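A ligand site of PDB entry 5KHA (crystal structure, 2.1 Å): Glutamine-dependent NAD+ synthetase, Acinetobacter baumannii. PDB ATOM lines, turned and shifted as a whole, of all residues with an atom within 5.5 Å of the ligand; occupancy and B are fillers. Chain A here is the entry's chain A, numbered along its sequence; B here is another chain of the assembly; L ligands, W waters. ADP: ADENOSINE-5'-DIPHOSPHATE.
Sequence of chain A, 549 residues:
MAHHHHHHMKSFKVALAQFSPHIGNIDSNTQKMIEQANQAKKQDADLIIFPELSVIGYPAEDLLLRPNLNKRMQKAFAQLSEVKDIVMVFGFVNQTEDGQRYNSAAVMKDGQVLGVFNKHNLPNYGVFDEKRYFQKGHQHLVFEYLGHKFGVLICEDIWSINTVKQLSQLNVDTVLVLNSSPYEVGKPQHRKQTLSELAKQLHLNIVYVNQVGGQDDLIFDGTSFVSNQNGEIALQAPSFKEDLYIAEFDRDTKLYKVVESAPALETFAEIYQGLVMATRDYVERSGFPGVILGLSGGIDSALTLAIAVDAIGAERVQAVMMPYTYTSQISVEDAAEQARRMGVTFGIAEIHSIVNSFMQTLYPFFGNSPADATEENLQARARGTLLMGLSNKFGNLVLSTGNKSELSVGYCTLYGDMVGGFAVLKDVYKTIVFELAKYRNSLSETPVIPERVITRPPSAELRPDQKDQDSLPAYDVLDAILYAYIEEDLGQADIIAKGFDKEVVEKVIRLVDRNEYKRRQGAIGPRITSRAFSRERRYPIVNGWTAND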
ATOM      1  N   TYR A 282       9.958 -27.479  22.184  1.00  0.00           N
ATOM      2  CA  TYR A 282      10.483 -26.747  21.036  1.00  0.00           C
ATOM      3  C   TYR A 282       9.440 -26.667  19.916  1.00  0.00           C
ATOM      4  O   TYR A 282       9.258 -25.609  19.296  1.00  0.00           O
ATOM      5  CB  TYR A 282      11.782 -27.381  20.516  1.00  0.00           C
ATOM      6  CG  TYR A 282      12.464 -26.464  19.518  1.00  0.00           C
ATOM      7  CD1 TYR A 282      13.223 -25.372  19.956  1.00  0.00           C
ATOM      8  CD2 TYR A 282      12.295 -26.642  18.130  1.00  0.00           C
ATOM      9  CE1 TYR A 282      13.831 -24.486  19.036  1.00  0.00           C
ATOM     10  CE2 TYR A 282      12.921 -25.768  17.202  1.00  0.00           C
ATOM     11  CZ  TYR A 282      13.682 -24.698  17.665  1.00  0.00           C
ATOM     12  OH  TYR A 282      14.287 -23.811  16.774  1.00  0.00           O
ATOM     13  N   SER A 286       7.676 -22.942  19.302  1.00  0.00           N
ATOM     14  CA  SER A 286       7.941 -22.341  18.005  1.00  0.00           C
ATOM     15  C   SER A 286       6.705 -22.306  17.128  1.00  0.00           C
ATOM     16  O   SER A 286       6.746 -21.723  16.042  1.00  0.00           O
ATOM     17  CB  SER A 286       9.072 -23.118  17.309  1.00  0.00           C
ATOM     18  OG  SER A 286      10.148 -23.324  18.200  1.00  0.00           O
ATOM     19  N   PHE A 288       5.000 -24.834  15.506  1.00  0.00           N
ATOM     20  CA  PHE A 288       4.975 -25.724  14.329  1.00  0.00           C
ATOM     21  C   PHE A 288       3.697 -26.560  14.299  1.00  0.00           C
ATOM     22  O   PHE A 288       3.254 -27.051  15.347  1.00  0.00           O
ATOM     23  CB  PHE A 288       6.182 -26.662  14.334  1.00  0.00           C
ATOM     24  CG  PHE A 288       7.463 -26.028  13.891  1.00  0.00           C
ATOM     25  CD1 PHE A 288       7.730 -25.824  12.539  1.00  0.00           C
ATOM     26  CD2 PHE A 288       8.442 -25.692  14.824  1.00  0.00           C
ATOM     27  CE1 PHE A 288       8.932 -25.257  12.141  1.00  0.00           C
ATOM     28  CE2 PHE A 288       9.637 -25.124  14.433  1.00  0.00           C
ATOM     29  CZ  PHE A 288       9.880 -24.911  13.081  1.00  0.00           C
ATOM     30  N   MET A 388      13.504 -30.769   3.200  1.00  0.00           N
ATOM     31  CA  MET A 388      13.308 -29.319   3.298  1.00  0.00           C
ATOM     32  C   MET A 388      12.336 -28.809   2.239  1.00  0.00           C
ATOM     33  O   MET A 388      11.727 -27.754   2.418  1.00  0.00           O
ATOM     34  CB  MET A 388      14.643 -28.578   3.190  1.00  0.00           C
ATOM     35  CG  MET A 388      15.517 -28.741   4.425  1.00  0.00           C
ATOM     36  SD  MET A 388      14.737 -28.109   5.952  1.00  0.00           S
ATOM     37  CE  MET A 388      14.681 -26.353   5.640  1.00  0.00           C
ATOM     38  N   SER A 391       9.165 -29.544   4.110  1.00  0.00           N
ATOM     39  CA  SER A 391       9.059 -28.604   5.215  1.00  0.00           C
ATOM     40  C   SER A 391       8.657 -27.209   4.710  1.00  0.00           C
ATOM     41  O   SER A 391       7.703 -26.611   5.214  1.00  0.00           O
ATOM     42  CB  SER A 391      10.376 -28.556   5.979  1.00  0.00           C
ATOM     43  OG  SER A 391      10.313 -27.638   7.046  1.00  0.00           O
ATOM     44  N   ASN A 392       9.377 -26.711   3.695  1.00  0.00           N
ATOM     45  CA  ASN A 392       9.062 -25.404   3.108  1.00  0.00           C
ATOM     46  C   ASN A 392       7.612 -25.331   2.645  1.00  0.00           C
ATOM     47  O   ASN A 392       6.948 -24.307   2.843  1.00  0.00           O
ATOM     48  CB  ASN A 392       9.987 -25.092   1.923  1.00  0.00           C
ATOM     49  CG  ASN A 392      11.418 -24.797   2.357  1.00  0.00           C
ATOM     50  OD1 ASN A 392      11.702 -24.566   3.549  1.00  0.00           O
ATOM     51  ND2 ASN A 392      12.336 -24.798   1.390  1.00  0.00           N
ATOM     52  N   ASN A 396       6.145 -28.418   8.364  1.00  0.00           N
ATOM     53  CA  ASN A 396       6.628 -29.249   9.470  1.00  0.00           C
ATOM     54  C   ASN A 396       8.084 -28.956   9.786  1.00  0.00           C
ATOM     55  O   ASN A 396       8.897 -28.722   8.892  1.00  0.00           O
ATOM     56  CB  ASN A 396       6.475 -30.734   9.147  1.00  0.00           C
ATOM     57  CG  ASN A 396       5.033 -31.190   9.162  1.00  0.00           C
ATOM     58  OD1 ASN A 396       4.208 -30.658   9.904  1.00  0.00           O
ATOM     59  ND2 ASN A 396       4.710 -32.133   8.291  1.00  0.00           N
ATOM     60  N   LEU A 397       8.397 -28.949  11.089  1.00  0.00           N
ATOM     61  CA  LEU A 397       9.773 -28.925  11.547  1.00  0.00           C
ATOM     62  C   LEU A 397      10.477 -30.223  11.181  1.00  0.00           C
ATOM     63  O   LEU A 397       9.946 -31.314  11.441  1.00  0.00           O
ATOM     64  CB  LEU A 397       9.798 -28.738  13.079  1.00  0.00           C
ATOM     65  CG  LEU A 397      11.134 -28.976  13.784  1.00  0.00           C
ATOM     66  CD1 LEU A 397      12.102 -27.821  13.405  1.00  0.00           C
ATOM     67  CD2 LEU A 397      10.958 -29.040  15.309  1.00  0.00           C
ATOM     68  N   VAL A 398      11.657 -30.130  10.579  1.00  0.00           N
ATOM     69  CA  VAL A 398      12.439 -31.325  10.276  1.00  0.00           C
ATOM     70  C   VAL A 398      13.242 -31.739  11.510  1.00  0.00           C
ATOM     71  O   VAL A 398      14.049 -30.960  12.021  1.00  0.00           O
ATOM     72  CB  VAL A 398      13.374 -31.106   9.076  1.00  0.00           C
ATOM     73  CG1 VAL A 398      14.248 -32.339   8.857  1.00  0.00           C
ATOM     74  CG2 VAL A 398      12.578 -30.802   7.811  1.00  0.00           C
ATOM     75  N   GLY A 421      15.779 -28.725  12.000  1.00  0.00           N
ATOM     76  CA  GLY A 421      15.642 -27.579  12.878  1.00  0.00           C
ATOM     77  C   GLY A 421      15.771 -27.927  14.358  1.00  0.00           C
ATOM     78  O   GLY A 421      15.875 -27.028  15.196  1.00  0.00           O
ATOM     79  N   PHE A 422      15.731 -29.218  14.683  1.00  0.00           N
ATOM     80  CA  PHE A 422      15.917 -29.678  16.062  1.00  0.00           C
ATOM     81  C   PHE A 422      16.496 -31.081  16.028  1.00  0.00           C
ATOM     82  O   PHE A 422      16.002 -31.930  15.278  1.00  0.00           O
ATOM     83  CB  PHE A 422      14.577 -29.676  16.832  1.00  0.00           C
ATOM     84  CG  PHE A 422      14.725 -29.813  18.337  1.00  0.00           C
ATOM     85  CD1 PHE A 422      15.188 -28.759  19.115  1.00  0.00           C
ATOM     86  CD2 PHE A 422      14.352 -30.998  18.968  1.00  0.00           C
ATOM     87  CE1 PHE A 422      15.293 -28.884  20.508  1.00  0.00           C
ATOM     88  CE2 PHE A 422      14.453 -31.136  20.358  1.00  0.00           C
ATOM     89  CZ  PHE A 422      14.927 -30.061  21.129  1.00  0.00           C
ATOM     90  N   ARG A 514      12.817 -13.687  14.235  1.00  0.00           N
ATOM     91  CA  ARG A 514      12.335 -14.970  13.724  1.00  0.00           C
ATOM     92  C   ARG A 514      13.453 -15.775  13.068  1.00  0.00           C
ATOM     93  O   ARG A 514      13.336 -16.996  12.967  1.00  0.00           O
ATOM     94  CB  ARG A 514      11.174 -14.773  12.739  1.00  0.00           C
ATOM     95  N   ASN A 515      14.536 -15.128  12.643  1.00  0.00           N
ATOM     96  CA  ASN A 515      15.596 -15.835  11.954  1.00  0.00           C
ATOM     97  C   ASN A 515      16.833 -16.075  12.814  1.00  0.00           C
ATOM     98  O   ASN A 515      17.913 -16.346  12.267  1.00  0.00           O
ATOM     99  CB  ASN A 515      15.943 -15.125  10.656  1.00  0.00           C
ATOM    100  CG  ASN A 515      14.888 -15.368   9.580  1.00  0.00           C
ATOM    101  OD1 ASN A 515      14.782 -16.491   9.063  1.00  0.00           O
ATOM    102  ND2 ASN A 515      14.082 -14.357   9.283  1.00  0.00           N
ATOM    103  N   TYR A 517      17.149 -18.798  14.677  1.00  0.00           N
ATOM    104  CA  TYR A 517      17.471 -20.213  14.469  1.00  0.00           C
ATOM    105  C   TYR A 517      18.299 -20.414  13.191  1.00  0.00           C
ATOM    106  O   TYR A 517      19.180 -21.276  13.146  1.00  0.00           O
ATOM    107  CB  TYR A 517      16.192 -21.059  14.389  1.00  0.00           C
ATOM    108  CG  TYR A 517      15.551 -20.932  13.020  1.00  0.00           C
ATOM    109  CD1 TYR A 517      14.818 -19.784  12.687  1.00  0.00           C
ATOM    110  CD2 TYR A 517      15.719 -21.922  12.060  1.00  0.00           C
ATOM    111  CE1 TYR A 517      14.245 -19.646  11.424  1.00  0.00           C
ATOM    112  CE2 TYR A 517      15.161 -21.778  10.781  1.00  0.00           C
ATOM    113  CZ  TYR A 517      14.422 -20.650  10.479  1.00  0.00           C
ATOM    114  OH  TYR A 517      13.856 -20.517   9.227  1.00  0.00           O
ATOM    115  N   LYS A 518      18.032 -19.614  12.147  1.00  0.00           N
ATOM    116  CA  LYS A 518      18.697 -19.823  10.854  1.00  0.00           C
ATOM    117  C   LYS A 518      20.150 -19.376  10.891  1.00  0.00           C
ATOM    118  O   LYS A 518      21.035 -20.086  10.407  1.00  0.00           O
ATOM    119  CB  LYS A 518      17.928 -19.088   9.743  1.00  0.00           C
ATOM    120  CG  LYS A 518      18.584 -19.203   8.365  1.00  0.00           C
ATOM    121  CD  LYS A 518      17.770 -18.465   7.276  1.00  0.00           C
ATOM    122  CE  LYS A 518      16.490 -19.211   6.917  1.00  0.00           C
ATOM    123  NZ  LYS A 518      15.681 -18.523   5.864  1.00  0.00           N
ATOM    124  N   ILE A 541      16.622 -18.646  21.002  1.00  0.00           N
ATOM    125  CA  ILE A 541      15.813 -18.967  19.819  1.00  0.00           C
ATOM    126  C   ILE A 541      14.325 -18.862  20.162  1.00  0.00           C
ATOM    127  O   ILE A 541      13.596 -18.067  19.564  1.00  0.00           O
ATOM    128  CB  ILE A 541      16.167 -20.353  19.257  1.00  0.00           C
ATOM    129  CG1 ILE A 541      17.585 -20.351  18.675  1.00  0.00           C
ATOM    130  CG2 ILE A 541      15.165 -20.727  18.166  1.00  0.00           C
ATOM    131  CD1 ILE A 541      18.296 -21.695  18.737  1.00  0.00           C
ATOM    132  N   ALA B 373       8.084 -20.110  -2.607  1.00  0.00           N
ATOM    133  CA  ALA B 373       9.508 -20.117  -2.313  1.00  0.00           C
ATOM    134  C   ALA B 373      10.100 -21.525  -2.413  1.00  0.00           C
ATOM    135  O   ALA B 373      11.295 -21.656  -2.722  1.00  0.00           O
ATOM    136  CB  ALA B 373       9.748 -19.525  -0.928  1.00  0.00           C
ATOM    137  N   ASN B 377      13.788 -22.376  -3.545  1.00  0.00           N
ATOM    138  CA  ASN B 377      14.728 -22.916  -2.571  1.00  0.00           C
ATOM    139  C   ASN B 377      15.449 -24.149  -3.099  1.00  0.00           C
ATOM    140  O   ASN B 377      16.627 -24.366  -2.782  1.00  0.00           O
ATOM    141  CB  ASN B 377      14.008 -23.223  -1.263  1.00  0.00           C
ATOM    142  CG  ASN B 377      13.534 -21.972  -0.541  1.00  0.00           C
ATOM    143  OD1 ASN B 377      14.007 -20.872  -0.814  1.00  0.00           O
ATOM    144  ND2 ASN B 377      12.580 -22.140   0.350  1.00  0.00           N
ATOM    145  N   ARG B 381      19.523 -25.033  -3.124  1.00  0.00           N
ATOM    146  CA  ARG B 381      20.082 -26.250  -2.536  1.00  0.00           C
ATOM    147  C   ARG B 381      20.813 -27.094  -3.568  1.00  0.00           C
ATOM    148  O   ARG B 381      21.855 -27.684  -3.259  1.00  0.00           O
ATOM    149  CB  ARG B 381      18.966 -27.042  -1.849  1.00  0.00           C
ATOM    150  CG  ARG B 381      18.549 -26.299  -0.589  1.00  0.00           C
ATOM    151  CD  ARG B 381      17.489 -26.962   0.279  1.00  0.00           C
ATOM    152  NE  ARG B 381      17.292 -26.102   1.433  1.00  0.00           N
ATOM    153  CZ  ARG B 381      16.167 -25.452   1.727  1.00  0.00           C
ATOM    154  NH1 ARG B 381      15.096 -25.588   0.960  1.00  0.00           N
ATOM    155  NH2 ARG B 381      16.128 -24.673   2.793  1.00  0.00           N
ATOM    156  N   GLY B 410      16.745 -13.184   7.318  1.00  0.00           N
ATOM    157  CA  GLY B 410      16.488 -14.515   6.800  1.00  0.00           C
ATOM    158  C   GLY B 410      16.266 -14.575   5.294  1.00  0.00           C
ATOM    159  O   GLY B 410      15.571 -15.484   4.830  1.00  0.00           O
ATOM    160  N   CYS B 412      17.881 -15.753   2.939  1.00  0.00           N
ATOM    161  CA  CYS B 412      18.888 -16.735   2.600  1.00  0.00           C
ATOM    162  C   CYS B 412      18.253 -18.102   2.786  1.00  0.00           C
ATOM    163  O   CYS B 412      17.234 -18.248   3.466  1.00  0.00           O
ATOM    164  CB  CYS B 412      20.150 -16.580   3.451  1.00  0.00           C
ATOM    165  SG  CYS B 412      19.800 -16.288   5.197  1.00  0.00           S
ATOM    166  N   THR B 413      18.840 -19.088   2.136  1.00  0.00           N
ATOM    167  CA  THR B 413      18.278 -20.430   2.177  1.00  0.00           C
ATOM    168  C   THR B 413      19.200 -21.348   2.963  1.00  0.00           C
ATOM    169  O   THR B 413      20.387 -21.498   2.615  1.00  0.00           O
ATOM    170  CB  THR B 413      18.027 -20.953   0.778  1.00  0.00           C
ATOM    171  OG1 THR B 413      19.205 -20.717   0.001  1.00  0.00           O
ATOM    172  CG2 THR B 413      16.890 -20.196   0.147  1.00  0.00           C
ATOM    173  N   LEU B 414      18.648 -21.986   3.984  1.00  0.00           N
ATOM    174  CA  LEU B 414      19.364 -23.019   4.722  1.00  0.00           C
ATOM    175  C   LEU B 414      19.788 -24.116   3.761  1.00  0.00           C
ATOM    176  O   LEU B 414      18.994 -24.564   2.917  1.00  0.00           O
ATOM    177  CB  LEU B 414      18.461 -23.577   5.811  1.00  0.00           C
ATOM    178  CG  LEU B 414      18.399 -22.778   7.111  1.00  0.00           C
ATOM    179  CD1 LEU B 414      17.074 -23.064   7.769  1.00  0.00           C
ATOM    180  CD2 LEU B 414      19.533 -23.241   8.023  1.00  0.00           C
HETATM  181  PB  ADP L   1      13.026 -19.638   3.112  1.00  0.00           P
HETATM  182  O1B ADP L   1      13.290 -18.831   4.376  1.00  0.00           O
HETATM  183  O2B ADP L   1      11.567 -19.703   2.789  1.00  0.00           O
HETATM  184  O3B ADP L   1      13.888 -19.066   1.966  1.00  0.00           O
HETATM  185  PA  ADP L   1      14.496 -21.846   4.422  1.00  0.00           P
HETATM  186  O1A ADP L   1      15.921 -21.328   4.302  1.00  0.00           O
HETATM  187  O2A ADP L   1      14.477 -23.314   4.174  1.00  0.00           O
HETATM  188  O3A ADP L   1      13.582 -21.120   3.338  1.00  0.00           O
HETATM  189  O5' ADP L   1      13.876 -21.476   5.872  1.00  0.00           O
HETATM  190  C5' ADP L   1      12.568 -21.916   6.317  1.00  0.00           C
HETATM  191  C4' ADP L   1      12.635 -23.282   6.974  1.00  0.00           C
HETATM  192  O4' ADP L   1      13.351 -23.207   8.227  1.00  0.00           O
HETATM  193  C3' ADP L   1      11.286 -23.890   7.319  1.00  0.00           C
HETATM  194  O3' ADP L   1      10.727 -24.552   6.182  1.00  0.00           O
HETATM  195  C2' ADP L   1      11.636 -24.844   8.462  1.00  0.00           C
HETATM  196  O2' ADP L   1      12.119 -26.107   7.994  1.00  0.00           O
HETATM  197  C1' ADP L   1      12.776 -24.087   9.173  1.00  0.00           C
HETATM  198  N9  ADP L   1      12.378 -23.331  10.354  1.00  0.00           N
HETATM  199  C8  ADP L   1      11.570 -22.222  10.388  1.00  0.00           C
HETATM  200  N7  ADP L   1      11.422 -21.708  11.590  1.00  0.00           N
HETATM  201  C5  ADP L   1      12.176 -22.549  12.403  1.00  0.00           C
HETATM  202  C6  ADP L   1      12.426 -22.547  13.790  1.00  0.00           C
HETATM  203  N6  ADP L   1      11.898 -21.672  14.649  1.00  0.00           N
HETATM  204  N1  ADP L   1      13.231 -23.520  14.280  1.00  0.00           N
HETATM  205  C2  ADP L   1      13.734 -24.427  13.431  1.00  0.00           C
HETATM  206  N3  ADP L   1      13.568 -24.522  12.109  1.00  0.00           N
HETATM  207  C4  ADP L   1      12.761 -23.556  11.654  1.00  0.00           C
HETATM  208  O   HOH W   1       8.181 -23.781   6.499  1.00  0.00           O
HETATM  209  O   HOH W   2      16.430 -24.376  15.425  1.00  0.00           O
HETATM  210  O   HOH W   3      12.139 -21.902  17.370  1.00  0.00           O
HETATM  211  O   HOH W   4      15.603 -25.474  10.198  1.00  0.00           O
HETATM  212  O   HOH W   5       9.938 -20.589   7.759  1.00  0.00           O
HETATM  213  O   HOH W   6      13.006 -27.763   9.860  1.00  0.00           O
HETATM  214  O   HOH W   7      10.794 -18.622   6.031  1.00  0.00           O
HETATM  215  O   HOH W   8       9.851 -21.694   2.481  1.00  0.00           O
HETATM  216  O   HOH W   9      10.822 -19.087  13.016  1.00  0.00           O
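The guanidinium group of Arg 381 of chain B is in salt-bridge range of an oxygen (O2A) of the ligand (2.5 Å).
An oxygen (O2') of the ligand lies within hydrogen-bond range of the side-chain hydroxyl (OG) of Ser 391 (2.6 Å).
OH of Tyr 282 lies within hydrogen-bond range of N1 of the ligand (2.7 Å).
The side-chain amide oxygen (OD1) of Asn 392 sits at hydrogen-bond distance from an oxygen (O3') of the ligand, at 2.8 Å.
The backbone NH (N) of Leu 414 of chain B is in hydrogen-bond range of an oxygen (O1A) of the ligand, 2.8 Å away.
NZ of Lys 518 lies within salt-bridge range of O1B of the ligand (2.8 Å).
An oxygen (O4') of the ligand sits at hydrogen-bond distance from the side-chain hydroxyl (OH) of Tyr 517 (2.9 Å).
ND2 of Asn 377 of chain B is in hydrogen-bond range of O3A of the ligand, 3.3 Å away.
The guanidinium group (NE) of Arg 381 of chain B sits at hydrogen-bond distance from the backbone carbonyl oxygen (O) of Leu 414 of chain B (2.7 Å).
OG of Ser 286 sits at hydrogen-bond distance from O of Tyr 282 (2.7 Å).
The side-chain amide nitrogen of Asn 392 lies close to the side-chain amide nitrogen of Asn 377 of chain B (2.9 Å).
ND2 of Asn 392 sits close to O of Met 388 (3.2 Å).
O of Cys 412 of chain B sits at hydrogen-bond distance from NZ of Lys 518, 2.9 Å away.
The side-chain amino group of Lys 518 lies within hydrogen-bond range of the backbone carbonyl oxygen of Gly 410 of chain B, 3.2 Å away.
ND2 of Asn 377 of chain B sits close to O of Ala 373 of chain B (3.4 Å).
The backbone NH of Gly 421 lies within hydrogen-bond range of the backbone carbonyl oxygen of Val 398.
The backbone carbonyl oxygen of Cys 412 of chain B sits close to an oxygen (O1A) of the ligand, 3.5 Å away.
Phe 288 touches the ligand (CZ to C5, 3.4 Å).
Met 388 touches the ligand.
CD1 of Leu 397 touches C2 of the ligand (3.8 Å).
CA of Gly 421 touches C2 of the ligand, at 3.7 Å.
CA of Thr 413 of chain B touches O1A of the ligand, 3.3 Å away.
Hydrophobic or aromatic side chains that line the ligand: Tyr 282, Phe 288, Met 388, Leu 397, Tyr 517 and Leu 414 of chain B.
The nearest printed residue that does not touch the ligand is Gly 410 of chain B (4.1 Å).
Water W8 bridges an oxygen (O2B) of the ligand (2.6 Å) and the side-chain amide nitrogen of Asn 377 of chain B (3.5 Å).
Water W6 lies within hydrogen-bond range of O2' of the ligand and N of Val 398.
Water W1 lies within hydrogen-bond range of an oxygen (O3') of the ligand (2.7 Å) and the backbone carbonyl oxygen of Ser 391 (3.1 Å).
Water W3 lies within hydrogen-bond range of OG of Ser 286 (2.6 Å), N6 of the ligand (2.7 Å) and OH of Tyr 282 (2.9 Å).
Water W9 lies within hydrogen-bond range of a nitrogen (N7) of the ligand (3.0 Å) and the backbone carbonyl oxygen of Arg 514 (3.3 Å).
Water W2 bridges the side-chain hydroxyl (OH) of Tyr 282 (2.6 Å) and the backbone carbonyl oxygen (O) of Gly 421 (2.7 Å).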
